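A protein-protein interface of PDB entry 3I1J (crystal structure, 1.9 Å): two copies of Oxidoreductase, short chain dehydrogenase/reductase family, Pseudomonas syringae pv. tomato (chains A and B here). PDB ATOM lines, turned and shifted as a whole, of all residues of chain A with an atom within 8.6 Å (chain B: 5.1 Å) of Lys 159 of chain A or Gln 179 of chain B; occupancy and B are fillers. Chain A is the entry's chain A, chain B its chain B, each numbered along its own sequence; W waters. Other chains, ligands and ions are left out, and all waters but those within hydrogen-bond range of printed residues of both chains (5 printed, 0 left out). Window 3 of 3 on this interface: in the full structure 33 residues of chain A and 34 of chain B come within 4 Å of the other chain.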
ATOM      1  N   LEU A 111      19.505   5.003  11.995  1.00  0.00           N
ATOM      2  CA  LEU A 111      19.370   5.311  10.563  1.00  0.00           C
ATOM      3  C   LEU A 111      19.893   6.681  10.160  1.00  0.00           C
ATOM      4  O   LEU A 111      20.460   6.834   9.075  1.00  0.00           O
ATOM      5  CB  LEU A 111      17.919   5.126  10.105  1.00  0.00           C
ATOM      6  CG  LEU A 111      17.362   3.689  10.198  1.00  0.00           C
ATOM      7  CD1 LEU A 111      15.825   3.785  10.123  1.00  0.00           C
ATOM      8  CD2 LEU A 111      17.972   2.766   9.144  1.00  0.00           C
ATOM      9  N   SER A 153      16.463 -15.428   7.400  1.00  0.00           N
ATOM     10  CA  SER A 153      15.882 -14.199   7.903  1.00  0.00           C
ATOM     11  C   SER A 153      16.309 -13.981   9.353  1.00  0.00           C
ATOM     12  O   SER A 153      17.396 -14.431   9.770  1.00  0.00           O
ATOM     13  CB  SER A 153      14.363 -14.216   7.752  1.00  0.00           C
ATOM     14  OG  SER A 153      13.807 -12.905   7.941  1.00  0.00           O
ATOM     15  N   SER A 154      15.468 -13.285  10.113  1.00  0.00           N
ATOM     16  CA  SER A 154      15.811 -12.781  11.440  1.00  0.00           C
ATOM     17  C   SER A 154      14.522 -12.303  12.064  1.00  0.00           C
ATOM     18  O   SER A 154      13.583 -11.923  11.327  1.00  0.00           O
ATOM     19  CB  SER A 154      16.781 -11.591  11.285  1.00  0.00           C
ATOM     20  OG  SER A 154      16.923 -10.881  12.486  1.00  0.00           O
ATOM     21  N   SER A 155      14.450 -12.298  13.398  1.00  0.00           N
ATOM     22  CA  SER A 155      13.306 -11.648  14.062  1.00  0.00           C
ATOM     23  C   SER A 155      13.098 -10.196  13.556  1.00  0.00           C
ATOM     24  O   SER A 155      11.958  -9.723  13.452  1.00  0.00           O
ATOM     25  CB  SER A 155      13.425 -11.728  15.579  1.00  0.00           C
ATOM     26  OG  SER A 155      14.536 -11.006  16.060  1.00  0.00           O
ATOM     27  N   VAL A 156      14.197  -9.513  13.198  1.00  0.00           N
ATOM     28  CA  VAL A 156      14.116  -8.112  12.744  1.00  0.00           C
ATOM     29  C   VAL A 156      13.723  -7.972  11.283  1.00  0.00           C
ATOM     30  O   VAL A 156      13.553  -6.855  10.801  1.00  0.00           O
ATOM     31  CB  VAL A 156      15.374  -7.221  13.116  1.00  0.00           C
ATOM     32  CG1 VAL A 156      15.516  -7.134  14.625  1.00  0.00           C
ATOM     33  CG2 VAL A 156      16.675  -7.703  12.459  1.00  0.00           C
ATOM     34  N   GLY A 157      13.574  -9.105  10.590  1.00  0.00           N
ATOM     35  CA  GLY A 157      13.005  -9.136   9.250  1.00  0.00           C
ATOM     36  C   GLY A 157      11.514  -9.345   9.282  1.00  0.00           C
ATOM     37  O   GLY A 157      10.856  -9.321   8.239  1.00  0.00           O
ATOM     38  N   ARG A 158      10.982  -9.548  10.488  1.00  0.00           N
ATOM     39  CA  ARG A 158       9.577  -9.797  10.688  1.00  0.00           C
ATOM     40  C   ARG A 158       8.923  -8.738  11.569  1.00  0.00           C
ATOM     41  O   ARG A 158       7.747  -8.433  11.391  1.00  0.00           O
ATOM     42  CB  ARG A 158       9.387 -11.195  11.304  1.00  0.00           C
ATOM     43  CG  ARG A 158       9.874 -12.308  10.342  1.00  0.00           C
ATOM     44  CD  ARG A 158       9.900 -13.708  10.975  1.00  0.00           C
ATOM     45  NE  ARG A 158      10.505 -14.664  10.040  1.00  0.00           N
ATOM     46  CZ  ARG A 158      10.759 -15.938  10.325  1.00  0.00           C
ATOM     47  NH1 ARG A 158      10.499 -16.411  11.542  1.00  0.00           N
ATOM     48  NH2 ARG A 158      11.284 -16.723   9.398  1.00  0.00           N
ATOM     49  N   LYS A 159       9.666  -8.227  12.554  1.00  0.00           N
ATOM     50  CA  LYS A 159       9.257  -7.051  13.327  1.00  0.00           C
ATOM     51  C   LYS A 159      10.463  -6.144  13.533  1.00  0.00           C
ATOM     52  O   LYS A 159      11.428  -6.541  14.197  1.00  0.00           O
ATOM     53  CB  LYS A 159       8.625  -7.450  14.666  1.00  0.00           C
ATOM     54  CG  LYS A 159       8.347  -6.270  15.621  1.00  0.00           C
ATOM     55  CD  LYS A 159       7.289  -5.315  15.068  1.00  0.00           C
ATOM     56  CE  LYS A 159       7.307  -3.906  15.746  1.00  0.00           C
ATOM     57  NZ  LYS A 159       8.578  -3.107  15.491  1.00  0.00           N
ATOM     58  N   GLY A 160      10.398  -4.940  12.959  1.00  0.00           N
ATOM     59  CA  GLY A 160      11.536  -4.011  12.917  1.00  0.00           C
ATOM     60  C   GLY A 160      11.943  -3.515  14.288  1.00  0.00           C
ATOM     61  O   GLY A 160      11.108  -3.360  15.145  1.00  0.00           O
ATOM     62  N   ARG A 161      13.243  -3.292  14.481  1.00  0.00           N
ATOM     63  CA  ARG A 161      13.817  -2.842  15.760  1.00  0.00           C
ATOM     64  C   ARG A 161      14.895  -1.809  15.529  1.00  0.00           C
ATOM     65  O   ARG A 161      15.645  -1.896  14.545  1.00  0.00           O
ATOM     66  CB  ARG A 161      14.497  -4.018  16.462  1.00  0.00           C
ATOM     67  CG  ARG A 161      13.815  -4.552  17.659  1.00  0.00           C
ATOM     68  CD  ARG A 161      12.385  -4.946  17.383  1.00  0.00           C
ATOM     69  NE  ARG A 161      11.435  -4.310  18.303  1.00  0.00           N
ATOM     70  CZ  ARG A 161      11.748  -3.683  19.440  1.00  0.00           C
ATOM     71  NH1 ARG A 161      10.780  -3.147  20.196  1.00  0.00           N
ATOM     72  NH2 ARG A 161      13.014  -3.591  19.846  1.00  0.00           N
ATOM     73  N   ALA A 162      15.019  -0.890  16.484  1.00  0.00           N
ATOM     74  CA  ALA A 162      16.002   0.185  16.426  1.00  0.00           C
ATOM     75  C   ALA A 162      17.431  -0.308  16.226  1.00  0.00           C
ATOM     76  O   ALA A 162      17.825  -1.380  16.718  1.00  0.00           O
ATOM     77  CB  ALA A 162      15.928   1.057  17.677  1.00  0.00           C
ATOM     78  N   ASN A 163      18.188   0.501  15.499  1.00  0.00           N
ATOM     79  CA  ASN A 163      19.623   0.304  15.231  1.00  0.00           C
ATOM     80  C   ASN A 163      20.026  -0.963  14.490  1.00  0.00           C
ATOM     81  O   ASN A 163      21.153  -1.444  14.635  1.00  0.00           O
ATOM     82  CB  ASN A 163      20.457   0.437  16.501  1.00  0.00           C
ATOM     83  CG  ASN A 163      20.080   1.662  17.310  1.00  0.00           C
ATOM     84  OD1 ASN A 163      20.120   1.630  18.532  1.00  0.00           O
ATOM     85  ND2 ASN A 163      19.696   2.727  16.642  1.00  0.00           N
ATOM     86  N   TRP A 164      19.131  -1.484  13.671  1.00  0.00           N
ATOM     87  CA  TRP A 164      19.498  -2.605  12.823  1.00  0.00           C
ATOM     88  C   TRP A 164      19.913  -2.167  11.403  1.00  0.00           C
ATOM     89  O   TRP A 164      20.249  -2.998  10.544  1.00  0.00           O
ATOM     90  CB  TRP A 164      18.410  -3.680  12.866  1.00  0.00           C
ATOM     91  CG  TRP A 164      18.520  -4.506  14.122  1.00  0.00           C
ATOM     92  CD1 TRP A 164      17.808  -4.353  15.293  1.00  0.00           C
ATOM     93  CD2 TRP A 164      19.421  -5.586  14.334  1.00  0.00           C
ATOM     94  NE1 TRP A 164      18.208  -5.296  16.210  1.00  0.00           N
ATOM     95  CE2 TRP A 164      19.193  -6.074  15.646  1.00  0.00           C
ATOM     96  CE3 TRP A 164      20.408  -6.200  13.534  1.00  0.00           C
ATOM     97  CZ2 TRP A 164      19.920  -7.146  16.186  1.00  0.00           C
ATOM     98  CZ3 TRP A 164      21.115  -7.288  14.066  1.00  0.00           C
ATOM     99  CH2 TRP A 164      20.856  -7.749  15.383  1.00  0.00           C
ATOM    100  N   GLY A 168      17.898  -5.142   9.158  1.00  0.00           N
ATOM    101  CA  GLY A 168      16.461  -5.448   9.337  1.00  0.00           C
ATOM    102  C   GLY A 168      15.693  -5.230   8.023  1.00  0.00           C
ATOM    103  O   GLY A 168      14.896  -6.063   7.615  1.00  0.00           O
ATOM    104  N   VAL A 169      15.938  -4.091   7.388  1.00  0.00           N
ATOM    105  CA  VAL A 169      15.358  -3.743   6.089  1.00  0.00           C
ATOM    106  C   VAL A 169      15.601  -4.858   5.078  1.00  0.00           C
ATOM    107  O   VAL A 169      14.686  -5.253   4.376  1.00  0.00           O
ATOM    108  CB  VAL A 169      15.911  -2.382   5.547  1.00  0.00           C
ATOM    109  CG1 VAL A 169      15.257  -2.021   4.225  1.00  0.00           C
ATOM    110  CG2 VAL A 169      15.644  -1.264   6.556  1.00  0.00           C
ATOM    111  N   LYS A 171      16.211  -7.966   5.595  1.00  0.00           N
ATOM    112  CA  LYS A 171      15.512  -9.206   5.949  1.00  0.00           C
ATOM    113  C   LYS A 171      14.009  -9.122   5.726  1.00  0.00           C
ATOM    114  O   LYS A 171      13.384 -10.120   5.400  1.00  0.00           O
ATOM    115  CB  LYS A 171      15.905  -9.703   7.344  1.00  0.00           C
ATOM    116  CG  LYS A 171      17.426 -10.106   7.425  1.00  0.00           C
ATOM    117  CD  LYS A 171      17.774 -11.115   6.287  1.00  0.00           C
ATOM    118  CE  LYS A 171      19.244 -11.564   6.316  1.00  0.00           C
ATOM    119  NZ  LYS A 171      19.542 -12.704   5.431  1.00  0.00           N
ATOM    120  N   PHE A 172      13.450  -7.926   5.897  1.00  0.00           N
ATOM    121  CA  PHE A 172      12.081  -7.625   5.440  1.00  0.00           C
ATOM    122  C   PHE A 172      11.976  -7.881   3.931  1.00  0.00           C
ATOM    123  O   PHE A 172      11.057  -8.584   3.472  1.00  0.00           O
ATOM    124  CB  PHE A 172      11.691  -6.178   5.777  1.00  0.00           C
ATOM    125  CG  PHE A 172      10.878  -6.056   7.055  1.00  0.00           C
ATOM    126  CD1 PHE A 172      11.499  -5.993   8.290  1.00  0.00           C
ATOM    127  CD2 PHE A 172       9.495  -5.983   7.007  1.00  0.00           C
ATOM    128  CE1 PHE A 172      10.756  -5.885   9.466  1.00  0.00           C
ATOM    129  CE2 PHE A 172       8.741  -5.864   8.178  1.00  0.00           C
ATOM    130  CZ  PHE A 172       9.390  -5.810   9.416  1.00  0.00           C
ATOM    131  N   GLU A 175      11.928 -11.660   3.279  1.00  0.00           N
ATOM    132  CA  GLU A 175      10.647 -12.306   3.507  1.00  0.00           C
ATOM    133  C   GLU A 175       9.721 -12.008   2.351  1.00  0.00           C
ATOM    134  O   GLU A 175       8.986 -12.874   1.910  1.00  0.00           O
ATOM    135  CB  GLU A 175      10.000 -11.791   4.802  1.00  0.00           C
ATOM    136  CG  GLU A 175      10.822 -12.142   6.040  1.00  0.00           C
ATOM    137  CD  GLU A 175      10.755 -13.628   6.443  1.00  0.00           C
ATOM    138  OE1 GLU A 175      10.014 -14.448   5.819  1.00  0.00           O
ATOM    139  OE2 GLU A 175      11.438 -13.953   7.434  1.00  0.00           O
ATOM    140  N   THR B 174      10.390  -1.322   2.547  1.00  0.00           N
ATOM    141  CA  THR B 174       9.816  -0.060   3.036  1.00  0.00           C
ATOM    142  C   THR B 174       9.143  -0.188   4.404  1.00  0.00           C
ATOM    143  O   THR B 174       9.348   0.674   5.257  1.00  0.00           O
ATOM    144  CB  THR B 174       8.710   0.433   2.081  1.00  0.00           C
ATOM    145  OG1 THR B 174       9.280   0.776   0.835  1.00  0.00           O
ATOM    146  CG2 THR B 174       8.004   1.683   2.643  1.00  0.00           C
ATOM    147  N   GLU B 175       8.299  -1.219   4.592  1.00  0.00           N
ATOM    148  CA  GLU B 175       7.717  -1.459   5.910  1.00  0.00           C
ATOM    149  C   GLU B 175       8.801  -1.691   6.959  1.00  0.00           C
ATOM    150  O   GLU B 175       8.687  -1.194   8.066  1.00  0.00           O
ATOM    151  CB  GLU B 175       6.753  -2.661   5.930  1.00  0.00           C
ATOM    152  CG  GLU B 175       5.553  -2.615   4.980  1.00  0.00           C
ATOM    153  CD  GLU B 175       4.474  -1.579   5.355  1.00  0.00           C
ATOM    154  OE1 GLU B 175       4.580  -0.873   6.391  1.00  0.00           O
ATOM    155  OE2 GLU B 175       3.495  -1.473   4.571  1.00  0.00           O
ATOM    156  N   GLY B 176       9.836  -2.477   6.626  1.00  0.00           N
ATOM    157  CA  GLY B 176      10.930  -2.767   7.568  1.00  0.00           C
ATOM    158  C   GLY B 176      11.739  -1.514   7.912  1.00  0.00           C
ATOM    159  O   GLY B 176      12.159  -1.322   9.053  1.00  0.00           O
ATOM    160  N   LEU B 177      11.939  -0.656   6.921  1.00  0.00           N
ATOM    161  CA  LEU B 177      12.555   0.663   7.137  1.00  0.00           C
ATOM    162  C   LEU B 177      11.698   1.528   8.084  1.00  0.00           C
ATOM    163  O   LEU B 177      12.208   2.121   9.019  1.00  0.00           O
ATOM    164  CB  LEU B 177      12.693   1.416   5.814  1.00  0.00           C
ATOM    165  CG  LEU B 177      13.877   2.305   5.422  1.00  0.00           C
ATOM    166  CD1 LEU B 177      13.462   3.445   4.471  1.00  0.00           C
ATOM    167  CD2 LEU B 177      14.809   2.780   6.553  1.00  0.00           C
ATOM    168  N   MET B 178      10.406   1.599   7.817  1.00  0.00           N
ATOM    169  CA  MET B 178       9.499   2.393   8.662  1.00  0.00           C
ATOM    170  C   MET B 178       9.516   1.871  10.121  1.00  0.00           C
ATOM    171  O   MET B 178       9.564   2.667  11.084  1.00  0.00           O
ATOM    172  CB  MET B 178       8.077   2.397   8.086  1.00  0.00           C
ATOM    173  CG  MET B 178       7.035   3.185   8.944  1.00  0.00           C
ATOM    174  SD  MET B 178       6.270   2.072  10.410  1.00  0.00           S
ATOM    175  CE  MET B 178       5.284   0.870   9.280  1.00  0.00           C
ATOM    176  N   GLN B 179       9.458   0.543  10.276  1.00  0.00           N
ATOM    177  CA  GLN B 179       9.404  -0.070  11.618  1.00  0.00           C
ATOM    178  C   GLN B 179      10.709   0.177  12.395  1.00  0.00           C
ATOM    179  O   GLN B 179      10.669   0.545  13.562  1.00  0.00           O
ATOM    180  CB  GLN B 179       9.096  -1.568  11.543  1.00  0.00           C
ATOM    181  CG  GLN B 179       7.630  -1.834  11.228  1.00  0.00           C
ATOM    182  CD  GLN B 179       7.304  -3.325  11.182  1.00  0.00           C
ATOM    183  OE1 GLN B 179       6.467  -3.774  10.393  1.00  0.00           O
ATOM    184  NE2 GLN B 179       7.934  -4.082  12.036  1.00  0.00           N
ATOM    185  N   THR B 180      11.837   0.006  11.724  1.00  0.00           N
ATOM    186  CA  THR B 180      13.178   0.336  12.275  1.00  0.00           C
ATOM    187  C   THR B 180      13.188   1.809  12.708  1.00  0.00           C
ATOM    188  O   THR B 180      13.468   2.102  13.851  1.00  0.00           O
ATOM    189  CB  THR B 180      14.306   0.083  11.236  1.00  0.00           C
ATOM    190  OG1 THR B 180      14.244  -1.266  10.755  1.00  0.00           O
ATOM    191  CG2 THR B 180      15.682   0.336  11.836  1.00  0.00           C
ATOM    192  N   LEU B 181      12.825   2.718  11.806  1.00  0.00           N
ATOM    193  CA  LEU B 181      12.849   4.153  12.104  1.00  0.00           C
ATOM    194  C   LEU B 181      11.944   4.542  13.282  1.00  0.00           C
ATOM    195  O   LEU B 181      12.362   5.272  14.196  1.00  0.00           O
ATOM    196  CB  LEU B 181      12.452   4.964  10.865  1.00  0.00           C
ATOM    197  CG  LEU B 181      12.553   6.506  10.991  1.00  0.00           C
ATOM    198  CD1 LEU B 181      13.951   6.928  11.466  1.00  0.00           C
ATOM    199  CD2 LEU B 181      12.256   7.152   9.650  1.00  0.00           C
ATOM    200  N   ALA B 182      10.705   4.067  13.233  1.00  0.00           N
ATOM    201  CA  ALA B 182       9.737   4.288  14.296  1.00  0.00           C
ATOM    202  C   ALA B 182      10.279   3.863  15.671  1.00  0.00           C
ATOM    203  O   ALA B 182      10.135   4.596  16.649  1.00  0.00           O
ATOM    204  CB  ALA B 182       8.417   3.596  13.959  1.00  0.00           C
ATOM    205  N   ASP B 183      10.957   2.717  15.735  1.00  0.00           N
ATOM    206  CA  ASP B 183      11.530   2.259  16.993  1.00  0.00           C
ATOM    207  C   ASP B 183      12.665   3.185  17.503  1.00  0.00           C
ATOM    208  O   ASP B 183      12.855   3.350  18.705  1.00  0.00           O
ATOM    209  CB  ASP B 183      12.015   0.806  16.869  1.00  0.00           C
ATOM    210  CG  ASP B 183      12.129   0.107  18.232  1.00  0.00           C
ATOM    211  OD1 ASP B 183      11.299   0.382  19.088  1.00  0.00           O
ATOM    212  OD2 ASP B 183      13.039  -0.706  18.439  1.00  0.00           O
ATOM    213  N   GLY B 241       4.971   4.009  14.251  1.00  0.00           N
ATOM    214  CA  GLY B 241       5.227   2.606  13.965  1.00  0.00           C
ATOM    215  C   GLY B 241       4.032   1.866  13.403  1.00  0.00           C
ATOM    216  O   GLY B 241       4.001   0.632  13.411  1.00  0.00           O
HETATM  217  O   HOH W   1      14.880  -3.797  12.283  1.00  0.00           O
HETATM  218  O   HOH W   2       8.420  -0.061  15.204  1.00  0.00           O
HETATM  219  O   HOH W   3      15.064  -1.356  20.388  1.00  0.00           O
HETATM  220  O   HOH W   4      16.731  -2.478   9.885  1.00  0.00           O
HETATM  221  O   HOH W   5       5.707  -6.590  10.654  1.00  0.00           O
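Hydrophobic or aromatic side chains of chain A within 4 Å of the printed part of chain B: Leu 111, Ala 162, Val 169 and Phe 172.
Printed residues of chain B that touch a printed residue of chain A: Gly 176, Leu 177, Gln 179, Thr 180, Leu 181 and Asp 183.
Among the printed residues, Asp or Glu carboxylates within 4 Å of a Lys or Arg side-chain nitrogen of the other chain: Arg 161 of chain A with Asp 183 of chain B.
Position printed for both chains: 175.
Of the 11 pairs that touch across the chains among the printed residues, none has its exchanged pair printed and touching as well.
The side-chain hydroxyl of Thr 180 of chain B is in hydrogen-bond range of the backbone carbonyl oxygen of Gly 176 of chain B.
CD2 of Leu 177 of chain B touches CD1 of Leu 111 of chain A (3.8 Å).
Thr 180 of chain B touches Leu 111 of chain A (CG2 to CD1, 3.9 Å).
Leu 181 of chain B touches Leu 111 of chain A.
NE2 of Gln 179 of chain B touches CD of Lys 159 of chain A (3.3 Å).
O of Arg 161 of chain A touches CG2 of Thr 180 of chain B (3.5 Å).
Leu 177 of chain B touches Val 169 of chain A (CA to CG2, 3.7 Å).
Gly 176 of chain B touches Phe 172 of chain A (CA to CG, 3.3 Å).
NE2 of Gln 179 of chain B touches CZ of Phe 172 of chain A, 3.5 Å away.
Water W1 bridges N of Arg 161 of chain A (2.8 Å) and OG1 of Thr 180 of chain B (3.0 Å).
Water W5 lies within hydrogen-bond range of O of Arg 158 of chain A and OE1 of Gln 179 of chain B.
Water W2 bridges O of Gln 179 of chain B (2.8 Å) and NZ of Lys 159 of chain A (3.1 Å).
Water W3 lies within hydrogen-bond range of the side-chain carboxylate of Asp 183 of chain B (2.9 Å) and the guanidinium group of Arg 161 of chain A (3.1 Å).
Water W4 lies within hydrogen-bond range of the side-chain hydroxyl (OG1) of Thr 180 of chain B, the backbone NH (N) of Gly 168 of chain A and the backbone NH (N) of Val 169 of chain A.
Printed residues of chain B within 4 Å of Leu 111 of chain A: Leu 177, Thr 180 and Leu 181.
Of the printed residues of chain B, Phe 172 of chain A touches Gly 176 (3.3 Å) and Gln 179 (3.5 Å).
Of the printed residues of chain A, Thr 180 of chain B touches Leu 111 (3.9 Å) and Arg 161 (3.5 Å).
The nearest residue of chain A that does not touch Gln 179 of chain B is Arg 158 of chain A (4.4 Å).
The side-chain carboxylate (OD2) of Asp 183 of chain B lies within salt-bridge range of the guanidinium group (NH2) of Arg 161 of chain A, at 3.2 Å.
The side-chain amide nitrogen (NE2) of Gln 179 of chain B sits close to the backbone NH (N) of Gly 160 of chain A (2.8 Å).
The backbone NH (N) of Ala 162 of chain A sits at hydrogen-bond distance from the side-chain carboxylate (OD2) of Asp 183 of chain B, 2.8 Å away.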
